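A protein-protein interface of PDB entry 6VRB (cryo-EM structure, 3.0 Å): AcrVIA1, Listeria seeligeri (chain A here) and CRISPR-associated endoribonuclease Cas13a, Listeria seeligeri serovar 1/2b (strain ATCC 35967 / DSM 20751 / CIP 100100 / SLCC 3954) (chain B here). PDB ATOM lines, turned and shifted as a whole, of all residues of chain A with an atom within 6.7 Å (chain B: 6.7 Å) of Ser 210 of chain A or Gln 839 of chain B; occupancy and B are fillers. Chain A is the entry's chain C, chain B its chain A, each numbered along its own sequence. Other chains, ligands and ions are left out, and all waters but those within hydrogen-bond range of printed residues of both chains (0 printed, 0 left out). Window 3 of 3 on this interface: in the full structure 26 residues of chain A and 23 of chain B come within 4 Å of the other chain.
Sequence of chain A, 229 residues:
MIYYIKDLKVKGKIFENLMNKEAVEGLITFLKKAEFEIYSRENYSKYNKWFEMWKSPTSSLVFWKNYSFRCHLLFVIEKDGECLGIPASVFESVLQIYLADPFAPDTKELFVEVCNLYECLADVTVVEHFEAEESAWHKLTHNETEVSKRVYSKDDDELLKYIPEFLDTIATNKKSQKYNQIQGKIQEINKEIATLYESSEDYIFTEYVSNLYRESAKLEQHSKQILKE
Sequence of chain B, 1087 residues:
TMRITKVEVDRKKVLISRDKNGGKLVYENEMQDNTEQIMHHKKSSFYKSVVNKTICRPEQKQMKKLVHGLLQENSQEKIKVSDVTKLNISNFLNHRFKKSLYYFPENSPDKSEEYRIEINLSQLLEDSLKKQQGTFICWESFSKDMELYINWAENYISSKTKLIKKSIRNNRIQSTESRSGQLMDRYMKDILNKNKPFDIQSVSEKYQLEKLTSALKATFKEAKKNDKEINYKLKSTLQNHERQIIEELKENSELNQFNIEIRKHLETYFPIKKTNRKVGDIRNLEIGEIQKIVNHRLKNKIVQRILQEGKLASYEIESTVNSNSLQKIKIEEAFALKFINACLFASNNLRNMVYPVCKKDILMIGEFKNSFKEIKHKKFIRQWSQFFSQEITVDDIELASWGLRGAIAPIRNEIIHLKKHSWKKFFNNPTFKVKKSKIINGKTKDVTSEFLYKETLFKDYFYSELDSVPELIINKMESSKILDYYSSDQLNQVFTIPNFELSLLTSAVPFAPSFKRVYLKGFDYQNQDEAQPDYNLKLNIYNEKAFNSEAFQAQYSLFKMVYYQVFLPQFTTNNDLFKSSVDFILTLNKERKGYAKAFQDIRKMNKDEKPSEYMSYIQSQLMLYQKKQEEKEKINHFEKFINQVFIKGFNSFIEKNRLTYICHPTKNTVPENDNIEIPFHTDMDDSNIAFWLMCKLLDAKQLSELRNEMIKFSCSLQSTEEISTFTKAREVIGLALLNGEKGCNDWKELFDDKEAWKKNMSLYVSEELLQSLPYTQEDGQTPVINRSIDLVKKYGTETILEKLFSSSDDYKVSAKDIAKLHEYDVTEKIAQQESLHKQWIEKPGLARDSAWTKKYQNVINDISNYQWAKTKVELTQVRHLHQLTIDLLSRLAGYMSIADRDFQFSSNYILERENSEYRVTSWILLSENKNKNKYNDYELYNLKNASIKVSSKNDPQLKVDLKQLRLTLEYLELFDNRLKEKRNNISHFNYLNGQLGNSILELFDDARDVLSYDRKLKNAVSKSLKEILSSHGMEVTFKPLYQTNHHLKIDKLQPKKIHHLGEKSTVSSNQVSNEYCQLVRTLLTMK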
ATOM      1  N   TYR A 203     -27.011  16.506 -15.217  1.00  0.00           N
ATOM      2  CA  TYR A 203     -25.680  16.241 -14.599  1.00  0.00           C
ATOM      3  C   TYR A 203     -24.675  15.631 -15.590  1.00  0.00           C
ATOM      4  O   TYR A 203     -23.464  15.827 -15.389  1.00  0.00           O
ATOM      5  CB  TYR A 203     -25.807  15.456 -13.290  1.00  0.00           C
ATOM      6  CG  TYR A 203     -25.621  16.300 -12.053  1.00  0.00           C
ATOM      7  CD1 TYR A 203     -26.663  17.049 -11.534  1.00  0.00           C
ATOM      8  CD2 TYR A 203     -24.395  16.363 -11.412  1.00  0.00           C
ATOM      9  CE1 TYR A 203     -26.496  17.831 -10.403  1.00  0.00           C
ATOM     10  CE2 TYR A 203     -24.210  17.139 -10.282  1.00  0.00           C
ATOM     11  CZ  TYR A 203     -25.264  17.877  -9.774  1.00  0.00           C
ATOM     12  OH  TYR A 203     -25.092  18.646  -8.660  1.00  0.00           O
ATOM     13  N   ILE A 204     -25.146  14.887 -16.597  1.00  0.00           N
ATOM     14  CA  ILE A 204     -24.230  14.229 -17.578  1.00  0.00           C
ATOM     15  C   ILE A 204     -23.389  15.286 -18.308  1.00  0.00           C
ATOM     16  O   ILE A 204     -22.180  15.047 -18.495  1.00  0.00           O
ATOM     17  CB  ILE A 204     -25.010  13.327 -18.559  1.00  0.00           C
ATOM     18  CG1 ILE A 204     -26.154  14.075 -19.248  1.00  0.00           C
ATOM     19  CG2 ILE A 204     -25.504  12.072 -17.857  1.00  0.00           C
ATOM     20  CD1 ILE A 204     -26.835  13.281 -20.341  1.00  0.00           C
ATOM     21  N   PHE A 205     -23.994  16.425 -18.663  1.00  0.00           N
ATOM     22  CA  PHE A 205     -23.296  17.518 -19.388  1.00  0.00           C
ATOM     23  C   PHE A 205     -22.137  18.076 -18.550  1.00  0.00           C
ATOM     24  O   PHE A 205     -21.076  18.369 -19.133  1.00  0.00           O
ATOM     25  CB  PHE A 205     -24.287  18.621 -19.765  1.00  0.00           C
ATOM     26  CG  PHE A 205     -25.205  18.269 -20.909  1.00  0.00           C
ATOM     27  CD1 PHE A 205     -26.550  18.018 -20.689  1.00  0.00           C
ATOM     28  CD2 PHE A 205     -24.722  18.176 -22.204  1.00  0.00           C
ATOM     29  CE1 PHE A 205     -27.390  17.687 -21.740  1.00  0.00           C
ATOM     30  CE2 PHE A 205     -25.564  17.848 -23.253  1.00  0.00           C
ATOM     31  CZ  PHE A 205     -26.897  17.605 -23.021  1.00  0.00           C
ATOM     32  N   THR A 206     -22.317  18.175 -17.229  1.00  0.00           N
ATOM     33  CA  THR A 206     -21.277  18.762 -16.336  1.00  0.00           C
ATOM     34  C   THR A 206     -19.976  17.949 -16.376  1.00  0.00           C
ATOM     35  O   THR A 206     -20.042  16.715 -16.526  1.00  0.00           O
ATOM     36  CB  THR A 206     -21.787  18.953 -14.903  1.00  0.00           C
ATOM     37  OG1 THR A 206     -21.270  20.194 -14.421  1.00  0.00           O
ATOM     38  CG2 THR A 206     -21.376  17.828 -13.978  1.00  0.00           C
ATOM     39  N   GLU A 207     -18.842  18.652 -16.280  1.00  0.00           N
ATOM     40  CA  GLU A 207     -17.474  18.064 -16.323  1.00  0.00           C
ATOM     41  C   GLU A 207     -17.251  17.120 -15.136  1.00  0.00           C
ATOM     42  O   GLU A 207     -16.627  16.062 -15.339  1.00  0.00           O
ATOM     43  CB  GLU A 207     -16.425  19.178 -16.326  1.00  0.00           C
ATOM     44  CG  GLU A 207     -14.996  18.664 -16.335  1.00  0.00           C
ATOM     45  CD  GLU A 207     -14.695  17.622 -17.399  1.00  0.00           C
ATOM     46  OE1 GLU A 207     -13.655  17.748 -18.074  1.00  0.00           O
ATOM     47  OE2 GLU A 207     -15.498  16.681 -17.543  1.00  0.00           O
ATOM     48  N   TYR A 208     -17.783  17.465 -13.961  1.00  0.00           N
ATOM     49  CA  TYR A 208     -17.564  16.637 -12.745  1.00  0.00           C
ATOM     50  C   TYR A 208     -18.085  15.218 -12.995  1.00  0.00           C
ATOM     51  O   TYR A 208     -17.382  14.255 -12.629  1.00  0.00           O
ATOM     52  CB  TYR A 208     -18.272  17.278 -11.550  1.00  0.00           C
ATOM     53  CG  TYR A 208     -18.706  16.310 -10.480  1.00  0.00           C
ATOM     54  CD1 TYR A 208     -20.046  16.151 -10.164  1.00  0.00           C
ATOM     55  CD2 TYR A 208     -17.784  15.549  -9.781  1.00  0.00           C
ATOM     56  CE1 TYR A 208     -20.457  15.266  -9.183  1.00  0.00           C
ATOM     57  CE2 TYR A 208     -18.177  14.659  -8.796  1.00  0.00           C
ATOM     58  CZ  TYR A 208     -19.520  14.517  -8.496  1.00  0.00           C
ATOM     59  OH  TYR A 208     -19.922  13.643  -7.529  1.00  0.00           O
ATOM     60  N   VAL A 209     -19.252  15.094 -13.632  1.00  0.00           N
ATOM     61  CA  VAL A 209     -19.821  13.750 -13.948  1.00  0.00           C
ATOM     62  C   VAL A 209     -18.941  13.087 -15.014  1.00  0.00           C
ATOM     63  O   VAL A 209     -18.654  11.884 -14.882  1.00  0.00           O
ATOM     64  CB  VAL A 209     -21.288  13.847 -14.404  1.00  0.00           C
ATOM     65  CG1 VAL A 209     -21.698  12.645 -15.239  1.00  0.00           C
ATOM     66  CG2 VAL A 209     -22.228  14.028 -13.223  1.00  0.00           C
ATOM     67  N   SER A 210     -18.491  13.872 -16.000  1.00  0.00           N
ATOM     68  CA  SER A 210     -17.639  13.357 -17.103  1.00  0.00           C
ATOM     69  C   SER A 210     -16.330  12.812 -16.522  1.00  0.00           C
ATOM     70  O   SER A 210     -15.889  11.738 -16.965  1.00  0.00           O
ATOM     71  CB  SER A 210     -17.377  14.444 -18.113  1.00  0.00           C
ATOM     72  OG  SER A 210     -16.678  13.933 -19.237  1.00  0.00           O
ATOM     73  N   ASN A 211     -15.764  13.517 -15.541  1.00  0.00           N
ATOM     74  CA  ASN A 211     -14.503  13.088 -14.876  1.00  0.00           C
ATOM     75  C   ASN A 211     -14.738  11.749 -14.172  1.00  0.00           C
ATOM     76  O   ASN A 211     -13.864  10.869 -14.269  1.00  0.00           O
ATOM     77  CB  ASN A 211     -14.010  14.150 -13.892  1.00  0.00           C
ATOM     78  CG  ASN A 211     -13.641  15.451 -14.571  1.00  0.00           C
ATOM     79  OD1 ASN A 211     -12.943  15.452 -15.582  1.00  0.00           O
ATOM     80  ND2 ASN A 211     -14.103  16.564 -14.023  1.00  0.00           N
ATOM     81  N   LEU A 212     -15.907  11.590 -13.542  1.00  0.00           N
ATOM     82  CA  LEU A 212     -16.255  10.352 -12.794  1.00  0.00           C
ATOM     83  C   LEU A 212     -16.268   9.155 -13.753  1.00  0.00           C
ATOM     84  O   LEU A 212     -15.747   8.091 -13.366  1.00  0.00           O
ATOM     85  CB  LEU A 212     -17.628  10.546 -12.140  1.00  0.00           C
ATOM     86  CG  LEU A 212     -17.855   9.767 -10.844  1.00  0.00           C
ATOM     87  CD1 LEU A 212     -17.670   8.275 -11.067  1.00  0.00           C
ATOM     88  CD2 LEU A 212     -16.924  10.261  -9.748  1.00  0.00           C
ATOM     89  N   TYR A 213     -16.799   9.334 -14.968  1.00  0.00           N
ATOM     90  CA  TYR A 213     -16.849   8.222 -15.953  1.00  0.00           C
ATOM     91  C   TYR A 213     -15.419   7.774 -16.265  1.00  0.00           C
ATOM     92  O   TYR A 213     -15.167   6.557 -16.325  1.00  0.00           O
ATOM     93  CB  TYR A 213     -17.540   8.672 -17.243  1.00  0.00           C
ATOM     94  CG  TYR A 213     -19.045   8.616 -17.217  1.00  0.00           C
ATOM     95  CD1 TYR A 213     -19.712   7.409 -17.096  1.00  0.00           C
ATOM     96  CD2 TYR A 213     -19.806   9.766 -17.332  1.00  0.00           C
ATOM     97  CE1 TYR A 213     -21.096   7.346 -17.075  1.00  0.00           C
ATOM     98  CE2 TYR A 213     -21.190   9.722 -17.312  1.00  0.00           C
ATOM     99  CZ  TYR A 213     -21.838   8.507 -17.185  1.00  0.00           C
ATOM    100  OH  TYR A 213     -23.200   8.460 -17.169  1.00  0.00           O
ATOM    101  N   ARG A 214     -14.507   8.738 -16.418  1.00  0.00           N
ATOM    102  CA  ARG A 214     -13.085   8.415 -16.708  1.00  0.00           C
ATOM    103  C   ARG A 214     -12.539   7.512 -15.593  1.00  0.00           C
ATOM    104  O   ARG A 214     -11.838   6.539 -15.926  1.00  0.00           O
ATOM    105  CB  ARG A 214     -12.274   9.705 -16.852  1.00  0.00           C
ATOM    106  CG  ARG A 214     -12.735  10.589 -18.001  1.00  0.00           C
ATOM    107  CD  ARG A 214     -11.786  11.742 -18.268  1.00  0.00           C
ATOM    108  NE  ARG A 214     -12.183  12.528 -19.427  1.00  0.00           N
ATOM    109  CZ  ARG A 214     -11.458  13.507 -19.954  1.00  0.00           C
ATOM    110  NH1 ARG A 214     -10.290  13.825 -19.424  1.00  0.00           N
ATOM    111  NH2 ARG A 214     -11.904  14.167 -21.008  1.00  0.00           N
ATOM    112  N   GLU A 215     -12.875   7.796 -14.329  1.00  0.00           N
ATOM    113  CA  GLU A 215     -12.400   6.940 -13.245  1.00  0.00           C
ATOM    114  C   GLU A 215     -12.983   5.531 -13.369  1.00  0.00           C
ATOM    115  O   GLU A 215     -12.266   4.529 -13.209  1.00  0.00           O
ATOM    116  CB  GLU A 215     -12.746   7.534 -11.880  1.00  0.00           C
ATOM    117  CG  GLU A 215     -11.792   8.620 -11.415  1.00  0.00           C
ATOM    118  CD  GLU A 215     -11.824   8.814  -9.911  1.00  0.00           C
ATOM    119  OE1 GLU A 215     -12.452   7.985  -9.218  1.00  0.00           O
ATOM    120  OE2 GLU A 215     -11.220   9.791  -9.422  1.00  0.00           O
ATOM    121  N   GLU B 834     -23.128  17.347 -29.777  1.00  0.00           N
ATOM    122  CA  GLU B 834     -21.775  17.281 -30.306  1.00  0.00           C
ATOM    123  C   GLU B 834     -20.789  16.907 -29.211  1.00  0.00           C
ATOM    124  O   GLU B 834     -19.895  16.094 -29.427  1.00  0.00           O
ATOM    125  CB  GLU B 834     -21.374  18.615 -30.937  1.00  0.00           C
ATOM    126  CG  GLU B 834     -22.120  18.952 -32.215  1.00  0.00           C
ATOM    127  CD  GLU B 834     -21.563  20.182 -32.906  1.00  0.00           C
ATOM    128  OE1 GLU B 834     -20.683  20.848 -32.323  1.00  0.00           O
ATOM    129  OE2 GLU B 834     -22.006  20.484 -34.035  1.00  0.00           O
ATOM    130  N   SER B 835     -20.956  17.498 -28.033  1.00  0.00           N
ATOM    131  CA  SER B 835     -20.062  17.205 -26.921  1.00  0.00           C
ATOM    132  C   SER B 835     -20.170  15.750 -26.486  1.00  0.00           C
ATOM    133  O   SER B 835     -19.162  15.099 -26.220  1.00  0.00           O
ATOM    134  CB  SER B 835     -20.353  18.129 -25.741  1.00  0.00           C
ATOM    135  OG  SER B 835     -21.676  17.952 -25.274  1.00  0.00           O
ATOM    136  N   LEU B 836     -21.396  15.242 -26.410  1.00  0.00           N
ATOM    137  CA  LEU B 836     -21.611  13.858 -26.010  1.00  0.00           C
ATOM    138  C   LEU B 836     -21.023  12.881 -27.020  1.00  0.00           C
ATOM    139  O   LEU B 836     -20.407  11.887 -26.647  1.00  0.00           O
ATOM    140  CB  LEU B 836     -23.100  13.576 -25.810  1.00  0.00           C
ATOM    141  CG  LEU B 836     -23.754  14.269 -24.616  1.00  0.00           C
ATOM    142  CD1 LEU B 836     -25.196  13.816 -24.462  1.00  0.00           C
ATOM    143  CD2 LEU B 836     -22.967  13.987 -23.347  1.00  0.00           C
ATOM    144  N   HIS B 837     -21.211  13.173 -28.302  1.00  0.00           N
ATOM    145  CA  HIS B 837     -20.699  12.303 -29.351  1.00  0.00           C
ATOM    146  C   HIS B 837     -19.182  12.236 -29.337  1.00  0.00           C
ATOM    147  O   HIS B 837     -18.601  11.173 -29.529  1.00  0.00           O
ATOM    148  CB  HIS B 837     -21.193  12.732 -30.729  1.00  0.00           C
ATOM    149  CG  HIS B 837     -21.036  11.675 -31.775  1.00  0.00           C
ATOM    150  ND1 HIS B 837     -19.826  11.385 -32.366  1.00  0.00           N
ATOM    151  CD2 HIS B 837     -21.937  10.829 -32.329  1.00  0.00           C
ATOM    152  CE1 HIS B 837     -19.988  10.409 -33.241  1.00  0.00           C
ATOM    153  NE2 HIS B 837     -21.260  10.054 -33.238  1.00  0.00           N
ATOM    154  N   LYS B 838     -18.542  13.377 -29.100  1.00  0.00           N
ATOM    155  CA  LYS B 838     -17.084  13.439 -29.062  1.00  0.00           C
ATOM    156  C   LYS B 838     -16.533  12.576 -27.938  1.00  0.00           C
ATOM    157  O   LYS B 838     -15.522  11.897 -28.104  1.00  0.00           O
ATOM    158  CB  LYS B 838     -16.607  14.882 -28.900  1.00  0.00           C
ATOM    159  CG  LYS B 838     -16.778  15.732 -30.148  1.00  0.00           C
ATOM    160  CD  LYS B 838     -16.260  17.143 -29.925  1.00  0.00           C
ATOM    161  CE  LYS B 838     -16.397  17.984 -31.184  1.00  0.00           C
ATOM    162  NZ  LYS B 838     -15.636  17.400 -32.321  1.00  0.00           N
ATOM    163  N   GLN B 839     -17.203  12.606 -26.793  1.00  0.00           N
ATOM    164  CA  GLN B 839     -16.787  11.815 -25.648  1.00  0.00           C
ATOM    165  C   GLN B 839     -16.847  10.325 -25.952  1.00  0.00           C
ATOM    166  O   GLN B 839     -15.975   9.567 -25.533  1.00  0.00           O
ATOM    167  CB  GLN B 839     -17.659  12.123 -24.432  1.00  0.00           C
ATOM    168  CG  GLN B 839     -17.462  13.514 -23.857  1.00  0.00           C
ATOM    169  CD  GLN B 839     -18.181  13.699 -22.535  1.00  0.00           C
ATOM    170  OE1 GLN B 839     -18.842  12.786 -22.042  1.00  0.00           O
ATOM    171  NE2 GLN B 839     -18.050  14.884 -21.950  1.00  0.00           N
ATOM    172  N   TRP B 840     -17.873   9.901 -26.682  1.00  0.00           N
ATOM    173  CA  TRP B 840     -18.026   8.486 -26.972  1.00  0.00           C
ATOM    174  C   TRP B 840     -16.796   7.901 -27.662  1.00  0.00           C
ATOM    175  O   TRP B 840     -16.502   6.717 -27.474  1.00  0.00           O
ATOM    176  CB  TRP B 840     -19.284   8.272 -27.811  1.00  0.00           C
ATOM    177  CG  TRP B 840     -19.400   6.894 -28.298  1.00  0.00           C
ATOM    178  CD1 TRP B 840     -19.574   5.776 -27.557  1.00  0.00           C
ATOM    179  CD2 TRP B 840     -19.292   6.469 -29.653  1.00  0.00           C
ATOM    180  NE1 TRP B 840     -19.601   4.672 -28.368  1.00  0.00           N
ATOM    181  CE2 TRP B 840     -19.432   5.077 -29.664  1.00  0.00           C
ATOM    182  CE3 TRP B 840     -19.105   7.139 -30.864  1.00  0.00           C
ATOM    183  CZ2 TRP B 840     -19.384   4.341 -30.830  1.00  0.00           C
ATOM    184  CZ3 TRP B 840     -19.059   6.412 -32.015  1.00  0.00           C
ATOM    185  CH2 TRP B 840     -19.195   5.026 -31.996  1.00  0.00           C
ATOM    186  N   ILE B 841     -16.055   8.708 -28.429  1.00  0.00           N
ATOM    187  CA  ILE B 841     -14.881   8.194 -29.134  1.00  0.00           C
ATOM    188  C   ILE B 841     -13.780   7.804 -28.150  1.00  0.00           C
ATOM    189  O   ILE B 841     -13.189   6.722 -28.259  1.00  0.00           O
ATOM    190  CB  ILE B 841     -14.388   9.205 -30.193  1.00  0.00           C
ATOM    191  CG1 ILE B 841     -15.251   9.152 -31.459  1.00  0.00           C
ATOM    192  CG2 ILE B 841     -12.945   8.955 -30.584  1.00  0.00           C
ATOM    193  CD1 ILE B 841     -16.321  10.159 -31.561  1.00  0.00           C
ATOM    194  N   GLU B 842     -13.518   8.646 -27.145  1.00  0.00           N
ATOM    195  CA  GLU B 842     -12.467   8.306 -26.187  1.00  0.00           C
ATOM    196  C   GLU B 842     -12.908   7.219 -25.216  1.00  0.00           C
ATOM    197  O   GLU B 842     -12.082   6.426 -24.755  1.00  0.00           O
ATOM    198  CB  GLU B 842     -12.003   9.541 -25.425  1.00  0.00           C
ATOM    199  CG  GLU B 842     -11.016  10.371 -26.211  1.00  0.00           C
ATOM    200  CD  GLU B 842     -11.683  11.347 -27.131  1.00  0.00           C
ATOM    201  OE1 GLU B 842     -12.911  11.489 -27.029  1.00  0.00           O
ATOM    202  OE2 GLU B 842     -10.984  11.963 -27.959  1.00  0.00           O
ATOM    203  N   LYS B 843     -14.201   7.166 -24.890  1.00  0.00           N
ATOM    204  CA  LYS B 843     -14.687   6.123 -23.944  1.00  0.00           C
ATOM    205  C   LYS B 843     -15.814   5.333 -24.616  1.00  0.00           C
ATOM    206  O   LYS B 843     -16.987   5.623 -24.319  1.00  0.00           O
ATOM    207  CB  LYS B 843     -15.161   6.778 -22.642  1.00  0.00           C
ATOM    208  CG  LYS B 843     -14.703   6.090 -21.365  1.00  0.00           C
ATOM    209  CD  LYS B 843     -15.628   4.976 -20.925  1.00  0.00           C
ATOM    210  CE  LYS B 843     -16.555   5.385 -19.801  1.00  0.00           C
ATOM    211  NZ  LYS B 843     -17.132   4.208 -19.110  1.00  0.00           N
ATOM    212  N   PRO B 844     -15.525   4.351 -25.499  1.00  0.00           N
ATOM    213  CA  PRO B 844     -16.585   3.625 -26.214  1.00  0.00           C
ATOM    214  C   PRO B 844     -17.460   2.775 -25.316  1.00  0.00           C
ATOM    215  O   PRO B 844     -18.526   2.339 -25.765  1.00  0.00           O
ATOM    216  CB  PRO B 844     -15.806   2.750 -27.204  1.00  0.00           C
ATOM    217  CG  PRO B 844     -14.483   3.401 -27.327  1.00  0.00           C
ATOM    218  CD  PRO B 844     -14.190   3.959 -25.974  1.00  0.00           C
ATOM    219  N   LEU B 846     -19.196   3.910 -22.986  1.00  0.00           N
ATOM    220  CA  LEU B 846     -20.389   4.689 -22.675  1.00  0.00           C
ATOM    221  C   LEU B 846     -21.619   4.175 -23.406  1.00  0.00           C
ATOM    222  O   LEU B 846     -22.739   4.472 -22.986  1.00  0.00           O
ATOM    223  CB  LEU B 846     -20.183   6.160 -23.029  1.00  0.00           C
ATOM    224  CG  LEU B 846     -19.230   7.013 -22.202  1.00  0.00           C
ATOM    225  CD1 LEU B 846     -19.107   8.384 -22.826  1.00  0.00           C
ATOM    226  CD2 LEU B 846     -19.724   7.115 -20.781  1.00  0.00           C
ATOM    227  N   TRP B 852     -26.730   6.617 -19.725  1.00  0.00           N
ATOM    228  CA  TRP B 852     -26.053   7.565 -20.652  1.00  0.00           C
ATOM    229  C   TRP B 852     -26.687   7.518 -22.048  1.00  0.00           C
ATOM    230  O   TRP B 852     -26.920   8.595 -22.624  1.00  0.00           O
ATOM    231  CB  TRP B 852     -24.549   7.275 -20.707  1.00  0.00           C
ATOM    232  CG  TRP B 852     -23.749   8.358 -21.362  1.00  0.00           C
ATOM    233  CD1 TRP B 852     -23.154   9.424 -20.755  1.00  0.00           C
ATOM    234  CD2 TRP B 852     -23.455   8.480 -22.763  1.00  0.00           C
ATOM    235  NE1 TRP B 852     -22.511  10.201 -21.680  1.00  0.00           N
ATOM    236  CE2 TRP B 852     -22.677   9.646 -22.922  1.00  0.00           C
ATOM    237  CE3 TRP B 852     -23.772   7.722 -23.896  1.00  0.00           C
ATOM    238  CZ2 TRP B 852     -22.213  10.065 -24.166  1.00  0.00           C
ATOM    239  CZ3 TRP B 852     -23.313   8.137 -25.124  1.00  0.00           C
ATOM    240  CH2 TRP B 852     -22.545   9.295 -25.255  1.00  0.00           C
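The side-chain amide nitrogen (NE2) of Gln 839 of chain B sits at hydrogen-bond distance from the side-chain hydroxyl (OG) of Ser 210 of chain A, 3.2 Å away.
OE2 of Glu 207 of chain A sits close to OG of Ser 210 of chain A, at 3.4 Å.
Among the printed residues, merely in contact across the chains: Tyr 213 of chain A with Lys 843 of chain B, Tyr 213 of chain A with Leu 846 of chain B and Tyr 213 of chain A with Trp 852 of chain B.
Gln 839 of chain B touches just one residue of chain A: Ser 210.
Of the printed residues of chain A, Lys 843 of chain B touches Tyr 213 (3.9 Å).
Of the printed residues of chain B, Tyr 213 of chain A touches Lys 843 (3.9 Å), Leu 846 (3.7 Å) and Trp 852 (3.7 Å).
Of the printed residues of chain A, Trp 852 of chain B touches Tyr 213 (3.7 Å).
Of the printed residues of chain A, Leu 846 of chain B touches Tyr 213 (3.7 Å).
Pro 844 of chain B touches none of the printed residues of chain A.
The nearest printed residue of chain B that does not touch Tyr 213 of chain A is Gln 839 of chain B (5.7 Å).
Hydrophobic or aromatic side chains of chain A that line the printed part of chain B: Tyr 213.
Of the 13 printed residues of chain B, 4 touch a printed residue of chain A.
Among the printed residues, no Asp or Glu carboxylate lies within 4 Å of a Lys or Arg side-chain nitrogen of the other chain.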
